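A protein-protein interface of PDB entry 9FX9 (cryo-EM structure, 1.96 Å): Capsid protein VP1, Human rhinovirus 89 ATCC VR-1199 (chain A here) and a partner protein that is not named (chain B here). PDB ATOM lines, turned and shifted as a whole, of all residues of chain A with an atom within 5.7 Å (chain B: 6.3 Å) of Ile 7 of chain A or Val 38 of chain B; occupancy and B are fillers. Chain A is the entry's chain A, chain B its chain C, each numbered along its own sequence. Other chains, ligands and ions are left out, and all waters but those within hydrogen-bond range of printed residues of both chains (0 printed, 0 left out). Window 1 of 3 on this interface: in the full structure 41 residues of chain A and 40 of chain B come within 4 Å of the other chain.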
ATOM      1  N   THR A   5      23.469  -0.129 -25.991  1.00  0.00           N
ATOM      2  CA  THR A   5      23.666   1.059 -25.148  1.00  0.00           C
ATOM      3  C   THR A   5      25.010   1.087 -24.425  1.00  0.00           C
ATOM      4  O   THR A   5      25.245   2.002 -23.639  1.00  0.00           O
ATOM      5  CB  THR A   5      22.528   1.212 -24.137  1.00  0.00           C
ATOM      6  OG1 THR A   5      22.332   0.017 -23.434  1.00  0.00           O
ATOM      7  CG2 THR A   5      21.220   1.578 -24.806  1.00  0.00           C
ATOM      8  N   SER A   6      25.922   0.145 -24.671  1.00  0.00           N
ATOM      9  CA  SER A   6      27.316   0.295 -24.223  1.00  0.00           C
ATOM     10  C   SER A   6      27.942   1.553 -24.834  1.00  0.00           C
ATOM     11  O   SER A   6      27.560   1.977 -25.925  1.00  0.00           O
ATOM     12  CB  SER A   6      28.171  -0.927 -24.565  1.00  0.00           C
ATOM     13  OG  SER A   6      28.340  -1.056 -25.962  1.00  0.00           O
ATOM     14  N   ILE A   7      28.926   2.151 -24.165  1.00  0.00           N
ATOM     15  CA  ILE A   7      29.602   3.340 -24.704  1.00  0.00           C
ATOM     16  C   ILE A   7      30.322   3.037 -26.021  1.00  0.00           C
ATOM     17  O   ILE A   7      30.260   3.854 -26.935  1.00  0.00           O
ATOM     18  CB  ILE A   7      30.523   3.971 -23.640  1.00  0.00           C
ATOM     19  CG1 ILE A   7      29.711   4.594 -22.488  1.00  0.00           C
ATOM     20  CG2 ILE A   7      31.451   5.041 -24.228  1.00  0.00           C
ATOM     21  CD1 ILE A   7      28.644   5.622 -22.872  1.00  0.00           C
ATOM     22  N   GLU A   8      30.911   1.851 -26.178  1.00  0.00           N
ATOM     23  CA  GLU A   8      31.521   1.430 -27.445  1.00  0.00           C
ATOM     24  C   GLU A   8      30.485   1.416 -28.588  1.00  0.00           C
ATOM     25  O   GLU A   8      30.755   1.913 -29.671  1.00  0.00           O
ATOM     26  CB  GLU A   8      32.180   0.051 -27.273  1.00  0.00           C
ATOM     27  CG  GLU A   8      33.157  -0.332 -28.405  1.00  0.00           C
ATOM     28  CD  GLU A   8      34.586   0.241 -28.266  1.00  0.00           C
ATOM     29  OE1 GLU A   8      34.916   0.850 -27.230  1.00  0.00           O
ATOM     30  OE2 GLU A   8      35.402   0.046 -29.197  1.00  0.00           O
ATOM     31  N   SER A   9      29.269   0.923 -28.349  1.00  0.00           N
ATOM     32  CA  SER A   9      28.183   0.990 -29.333  1.00  0.00           C
ATOM     33  C   SER A   9      27.685   2.418 -29.580  1.00  0.00           C
ATOM     34  O   SER A   9      27.401   2.779 -30.719  1.00  0.00           O
ATOM     35  CB  SER A   9      27.015   0.108 -28.891  1.00  0.00           C
ATOM     36  OG  SER A   9      25.877   0.326 -29.703  1.00  0.00           O
ATOM     37  N   PHE A  10      27.542   3.237 -28.538  1.00  0.00           N
ATOM     38  CA  PHE A  10      26.961   4.571 -28.664  1.00  0.00           C
ATOM     39  C   PHE A  10      27.906   5.605 -29.298  1.00  0.00           C
ATOM     40  O   PHE A  10      27.479   6.372 -30.158  1.00  0.00           O
ATOM     41  CB  PHE A  10      26.462   5.027 -27.287  1.00  0.00           C
ATOM     42  CG  PHE A  10      25.817   6.392 -27.319  1.00  0.00           C
ATOM     43  CD1 PHE A  10      24.584   6.566 -27.973  1.00  0.00           C
ATOM     44  CD2 PHE A  10      26.451   7.490 -26.717  1.00  0.00           C
ATOM     45  CE1 PHE A  10      23.986   7.835 -28.008  1.00  0.00           C
ATOM     46  CE2 PHE A  10      25.862   8.759 -26.765  1.00  0.00           C
ATOM     47  CZ  PHE A  10      24.623   8.930 -27.408  1.00  0.00           C
ATOM     48  N   LEU A  11      29.182   5.631 -28.905  1.00  0.00           N
ATOM     49  CA  LEU A  11      30.192   6.564 -29.434  1.00  0.00           C
ATOM     50  C   LEU A  11      31.069   5.983 -30.556  1.00  0.00           C
ATOM     51  O   LEU A  11      31.686   6.746 -31.294  1.00  0.00           O
ATOM     52  CB  LEU A  11      31.080   7.072 -28.282  1.00  0.00           C
ATOM     53  CG  LEU A  11      30.376   7.910 -27.204  1.00  0.00           C
ATOM     54  CD1 LEU A  11      31.404   8.447 -26.211  1.00  0.00           C
ATOM     55  CD2 LEU A  11      29.644   9.108 -27.792  1.00  0.00           C
ATOM     56  N   GLY A  12      31.148   4.658 -30.690  1.00  0.00           N
ATOM     57  CA  GLY A  12      32.114   3.959 -31.546  1.00  0.00           C
ATOM     58  C   GLY A  12      31.599   3.529 -32.911  1.00  0.00           C
ATOM     59  O   GLY A  12      32.013   2.487 -33.421  1.00  0.00           O
ATOM     60  N   PHE A  58      29.278  13.507 -22.221  1.00  0.00           N
ATOM     61  CA  PHE A  58      30.327  13.154 -21.277  1.00  0.00           C
ATOM     62  C   PHE A  58      31.266  14.328 -21.064  1.00  0.00           C
ATOM     63  O   PHE A  58      31.386  15.216 -21.901  1.00  0.00           O
ATOM     64  CB  PHE A  58      31.061  11.909 -21.769  1.00  0.00           C
ATOM     65  CG  PHE A  58      30.096  10.788 -22.065  1.00  0.00           C
ATOM     66  CD1 PHE A  58      29.560  10.040 -21.009  1.00  0.00           C
ATOM     67  CD2 PHE A  58      29.639  10.582 -23.378  1.00  0.00           C
ATOM     68  CE1 PHE A  58      28.549   9.102 -21.263  1.00  0.00           C
ATOM     69  CE2 PHE A  58      28.634   9.642 -23.632  1.00  0.00           C
ATOM     70  CZ  PHE A  58      28.079   8.912 -22.571  1.00  0.00           C
ATOM     71  N   ILE A 188      36.795   2.744 -26.323  1.00  0.00           N
ATOM     72  CA  ILE A 188      36.275   3.998 -25.794  1.00  0.00           C
ATOM     73  C   ILE A 188      36.033   3.892 -24.294  1.00  0.00           C
ATOM     74  O   ILE A 188      35.415   2.942 -23.813  1.00  0.00           O
ATOM     75  CB  ILE A 188      34.995   4.451 -26.519  1.00  0.00           C
ATOM     76  CG1 ILE A 188      35.171   4.373 -28.044  1.00  0.00           C
ATOM     77  CG2 ILE A 188      34.627   5.888 -26.098  1.00  0.00           C
ATOM     78  CD1 ILE A 188      33.920   4.769 -28.811  1.00  0.00           C
ATOM     79  N   LYS A 189      36.455   4.914 -23.560  1.00  0.00           N
ATOM     80  CA  LYS A 189      36.060   5.167 -22.177  1.00  0.00           C
ATOM     81  C   LYS A 189      35.499   6.575 -22.073  1.00  0.00           C
ATOM     82  O   LYS A 189      35.949   7.476 -22.773  1.00  0.00           O
ATOM     83  CB  LYS A 189      37.243   4.913 -21.235  1.00  0.00           C
ATOM     84  CG  LYS A 189      37.603   3.423 -21.244  1.00  0.00           C
ATOM     85  CD  LYS A 189      38.725   3.088 -20.268  1.00  0.00           C
ATOM     86  CE  LYS A 189      38.991   1.580 -20.326  1.00  0.00           C
ATOM     87  NZ  LYS A 189      40.119   1.197 -19.450  1.00  0.00           N
ATOM     88  N   ALA A 190      34.498   6.755 -21.226  1.00  0.00           N
ATOM     89  CA  ALA A 190      33.814   8.024 -21.032  1.00  0.00           C
ATOM     90  C   ALA A 190      33.517   8.245 -19.551  1.00  0.00           C
ATOM     91  O   ALA A 190      33.203   7.299 -18.831  1.00  0.00           O
ATOM     92  CB  ALA A 190      32.550   8.055 -21.890  1.00  0.00           C
ATOM     93  N   TRP A 191      33.590   9.487 -19.090  1.00  0.00           N
ATOM     94  CA  TRP A 191      33.430   9.829 -17.678  1.00  0.00           C
ATOM     95  C   TRP A 191      32.558  11.059 -17.476  1.00  0.00           C
ATOM     96  O   TRP A 191      32.571  11.980 -18.295  1.00  0.00           O
ATOM     97  CB  TRP A 191      34.787  10.060 -17.012  1.00  0.00           C
ATOM     98  CG  TRP A 191      35.757   8.922 -16.994  1.00  0.00           C
ATOM     99  CD1 TRP A 191      35.966   8.099 -15.949  1.00  0.00           C
ATOM    100  CD2 TRP A 191      36.732   8.528 -18.005  1.00  0.00           C
ATOM    101  NE1 TRP A 191      36.984   7.220 -16.243  1.00  0.00           N
ATOM    102  CE2 TRP A 191      37.526   7.470 -17.479  1.00  0.00           C
ATOM    103  CE3 TRP A 191      37.065   8.994 -19.289  1.00  0.00           C
ATOM    104  CZ2 TRP A 191      38.610   6.922 -18.173  1.00  0.00           C
ATOM    105  CZ3 TRP A 191      38.152   8.451 -19.997  1.00  0.00           C
ATOM    106  CH2 TRP A 191      38.934   7.426 -19.439  1.00  0.00           C
ATOM    107  N   CYS A 192      31.887  11.091 -16.327  1.00  0.00           N
ATOM    108  CA  CYS A 192      31.107  12.202 -15.797  1.00  0.00           C
ATOM    109  C   CYS A 192      30.011  12.631 -16.782  1.00  0.00           C
ATOM    110  O   CYS A 192      30.221  13.564 -17.564  1.00  0.00           O
ATOM    111  CB  CYS A 192      32.057  13.327 -15.394  1.00  0.00           C
ATOM    112  SG  CYS A 192      33.138  12.793 -14.056  1.00  0.00           S
ATOM    113  N   PRO A 193      28.866  11.930 -16.789  1.00  0.00           N
ATOM    114  CA  PRO A 193      27.800  12.201 -17.732  1.00  0.00           C
ATOM    115  C   PRO A 193      27.193  13.584 -17.500  1.00  0.00           C
ATOM    116  O   PRO A 193      27.198  14.107 -16.389  1.00  0.00           O
ATOM    117  CB  PRO A 193      26.784  11.075 -17.564  1.00  0.00           C
ATOM    118  CG  PRO A 193      27.012  10.590 -16.139  1.00  0.00           C
ATOM    119  CD  PRO A 193      28.488  10.863 -15.877  1.00  0.00           C
ATOM    120  N   GLY B  36      33.435   8.511 -11.802  1.00  0.00           N
ATOM    121  CA  GLY B  36      32.235   8.637 -12.631  1.00  0.00           C
ATOM    122  C   GLY B  36      32.356   8.080 -14.043  1.00  0.00           C
ATOM    123  O   GLY B  36      31.780   8.649 -14.962  1.00  0.00           O
ATOM    124  N   GLN B  37      33.095   6.992 -14.252  1.00  0.00           N
ATOM    125  CA  GLN B  37      33.110   6.305 -15.544  1.00  0.00           C
ATOM    126  C   GLN B  37      31.710   5.789 -15.905  1.00  0.00           C
ATOM    127  O   GLN B  37      31.041   5.188 -15.070  1.00  0.00           O
ATOM    128  CB  GLN B  37      34.136   5.166 -15.538  1.00  0.00           C
ATOM    129  CG  GLN B  37      34.382   4.647 -16.965  1.00  0.00           C
ATOM    130  CD  GLN B  37      35.414   3.533 -17.094  1.00  0.00           C
ATOM    131  OE1 GLN B  37      35.529   2.902 -18.132  1.00  0.00           O
ATOM    132  NE2 GLN B  37      36.193   3.223 -16.085  1.00  0.00           N
ATOM    133  N   VAL B  38      31.285   5.979 -17.150  1.00  0.00           N
ATOM    134  CA  VAL B  38      30.049   5.413 -17.700  1.00  0.00           C
ATOM    135  C   VAL B  38      30.413   4.277 -18.643  1.00  0.00           C
ATOM    136  O   VAL B  38      31.235   4.461 -19.536  1.00  0.00           O
ATOM    137  CB  VAL B  38      29.219   6.479 -18.436  1.00  0.00           C
ATOM    138  CG1 VAL B  38      27.884   5.904 -18.918  1.00  0.00           C
ATOM    139  CG2 VAL B  38      28.923   7.677 -17.533  1.00  0.00           C
ATOM    140  N   ARG B  39      29.825   3.097 -18.462  1.00  0.00           N
ATOM    141  CA  ARG B  39      30.040   1.928 -19.335  1.00  0.00           C
ATOM    142  C   ARG B  39      28.829   1.663 -20.220  1.00  0.00           C
ATOM    143  O   ARG B  39      28.983   1.184 -21.341  1.00  0.00           O
ATOM    144  CB  ARG B  39      30.386   0.707 -18.477  1.00  0.00           C
ATOM    145  CG  ARG B  39      31.729   0.887 -17.752  1.00  0.00           C
ATOM    146  CD  ARG B  39      31.977  -0.266 -16.781  1.00  0.00           C
ATOM    147  NE  ARG B  39      33.219  -0.076 -16.013  1.00  0.00           N
ATOM    148  CZ  ARG B  39      33.365   0.623 -14.903  1.00  0.00           C
ATOM    149  NH1 ARG B  39      34.506   0.640 -14.289  1.00  0.00           N
ATOM    150  NH2 ARG B  39      32.394   1.315 -14.376  1.00  0.00           N
ATOM    151  N   ASN B  40      27.636   2.018 -19.752  1.00  0.00           N
ATOM    152  CA  ASN B  40      26.379   1.842 -20.468  1.00  0.00           C
ATOM    153  C   ASN B  40      25.453   3.052 -20.269  1.00  0.00           C
ATOM    154  O   ASN B  40      25.308   3.531 -19.150  1.00  0.00           O
ATOM    155  CB  ASN B  40      25.770   0.517 -19.974  1.00  0.00           C
ATOM    156  CG  ASN B  40      24.764  -0.056 -20.937  1.00  0.00           C
ATOM    157  OD1 ASN B  40      23.747   0.552 -21.224  1.00  0.00           O
ATOM    158  ND2 ASN B  40      25.016  -1.221 -21.481  1.00  0.00           N
ATOM    159  N   LEU B  41      24.757   3.525 -21.306  1.00  0.00           N
ATOM    160  CA  LEU B  41      23.784   4.619 -21.176  1.00  0.00           C
ATOM    161  C   LEU B  41      22.623   4.302 -20.227  1.00  0.00           C
ATOM    162  O   LEU B  41      22.039   5.216 -19.657  1.00  0.00           O
ATOM    163  CB  LEU B  41      23.177   4.992 -22.532  1.00  0.00           C
ATOM    164  CG  LEU B  41      24.119   5.624 -23.555  1.00  0.00           C
ATOM    165  CD1 LEU B  41      23.281   5.936 -24.786  1.00  0.00           C
ATOM    166  CD2 LEU B  41      24.752   6.914 -23.047  1.00  0.00           C
ATOM    167  N   GLU B  43      22.811   3.295 -17.284  1.00  0.00           N
ATOM    168  CA  GLU B  43      23.202   3.933 -16.016  1.00  0.00           C
ATOM    169  C   GLU B  43      22.683   5.377 -15.908  1.00  0.00           C
ATOM    170  O   GLU B  43      22.245   5.808 -14.845  1.00  0.00           O
ATOM    171  CB  GLU B  43      24.732   3.973 -15.888  1.00  0.00           C
ATOM    172  CG  GLU B  43      25.416   2.604 -15.961  1.00  0.00           C
ATOM    173  CD  GLU B  43      26.943   2.764 -15.929  1.00  0.00           C
ATOM    174  OE1 GLU B  43      27.467   3.277 -14.915  1.00  0.00           O
ATOM    175  OE2 GLU B  43      27.620   2.374 -16.901  1.00  0.00           O
ATOM    176  N   MET B  44      22.703   6.126 -17.011  1.00  0.00           N
ATOM    177  CA  MET B  44      22.200   7.498 -17.082  1.00  0.00           C
ATOM    178  C   MET B  44      20.672   7.525 -17.088  1.00  0.00           C
ATOM    179  O   MET B  44      20.081   8.342 -16.390  1.00  0.00           O
ATOM    180  CB  MET B  44      22.762   8.193 -18.327  1.00  0.00           C
ATOM    181  CG  MET B  44      24.288   8.313 -18.288  1.00  0.00           C
ATOM    182  SD  MET B  44      25.032   8.721 -19.880  1.00  0.00           S
ATOM    183  CE  MET B  44      24.237  10.298 -20.277  1.00  0.00           C
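CA of Ser 6 of chain A touches O of Arg 39 of chain B, at 3.4 Å.
Asn 40 of chain B touches Ser 6 of chain A (ND2 to N, 3.6 Å).
CG1 of Ile 7 of chain A touches O of Val 38 of chain B, at 3.3 Å.
Leu 41 of chain B touches Phe 58 of chain A (CD2 to CZ, 3.9 Å).
CE1 of Phe 58 of chain A touches SD of Met 44 of chain B, at 3.8 Å.
Lys 189 of chain A touches Gln 37 of chain B.
Ala 190 of chain A touches Gln 37 of chain B (O to CA, 3.4 Å).
CD1 of Trp 191 of chain A touches CA of Gln 37 of chain B (3.4 Å).
Pro 193 of chain A touches Val 38 of chain B.
SD of Met 44 of chain B touches CB of Pro 193 of chain A, 3.7 Å away.
The side-chain carboxylate (OE2) of Glu 43 of chain B lies within hydrogen-bond range of the backbone NH (N) of Arg 39 of chain B (2.8 Å).
N of Asn 40 of chain B lies within hydrogen-bond range of OE2 of Glu 43 of chain B, 2.9 Å away.
The side-chain hydroxyl (OG) of Ser 6 of chain A lies within hydrogen-bond range of the backbone NH (N) of Ser 9 of chain A, at 3.2 Å.
Of the 15 printed residues of chain A, 10 touch a printed residue of chain B.
Printed residues of chain A that touch a printed residue of chain B: Thr 5, Ser 6, Ile 7, Phe 10, Phe 58, Lys 189, Ala 190, Trp 191, Cys 192 and Pro 193.
Hydrophobic or aromatic side chains of chain A within 4 Å of the printed part of chain B: Ile 7, Phe 10, Phe 58, Trp 191 and Pro 193.
Among the printed residues, no Asp or Glu carboxylate lies within 4 Å of a Lys or Arg side-chain nitrogen of the other chain.
Ile 7 of chain A touches just these residues of chain B: Val 38 (3.3 Å) and Arg 39 (3.0 Å).
Of chain A, only Ile 7, Phe 58, Ala 190 and Pro 193 come within 4 Å of Val 38 of chain B.
Of the printed residues of chain B, Lys 189 of chain A touches Gln 37.
Of the printed residues of chain A, Met 44 of chain B touches Phe 58 and Pro 193.
Of the printed residues of chain B, Phe 58 of chain A touches Val 38, Leu 41 and Met 44.
The nearest printed residue of chain A that does not touch Gly 36 of chain B is Pro 193 of chain A (4.1 Å).
The backbone NH (N) of Cys 192 of chain A is in hydrogen-bond range of the backbone carbonyl oxygen (O) of Gly 36 of chain B, at 2.8 Å.
The side-chain amide oxygen of Asn 40 of chain B lies within hydrogen-bond range of the side-chain hydroxyl of Thr 5 of chain A, 2.7 Å away.
The backbone NH (N) of Ile 7 of chain A sits at hydrogen-bond distance from the backbone carbonyl oxygen (O) of Arg 39 of chain B, 3.0 Å away.
N of Leu 41 of chain B sits at hydrogen-bond distance from O of Thr 5 of chain A.
The backbone NH (N) of Val 38 of chain B is in hydrogen-bond range of the backbone carbonyl oxygen (O) of Ala 190 of chain A (2.9 Å).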
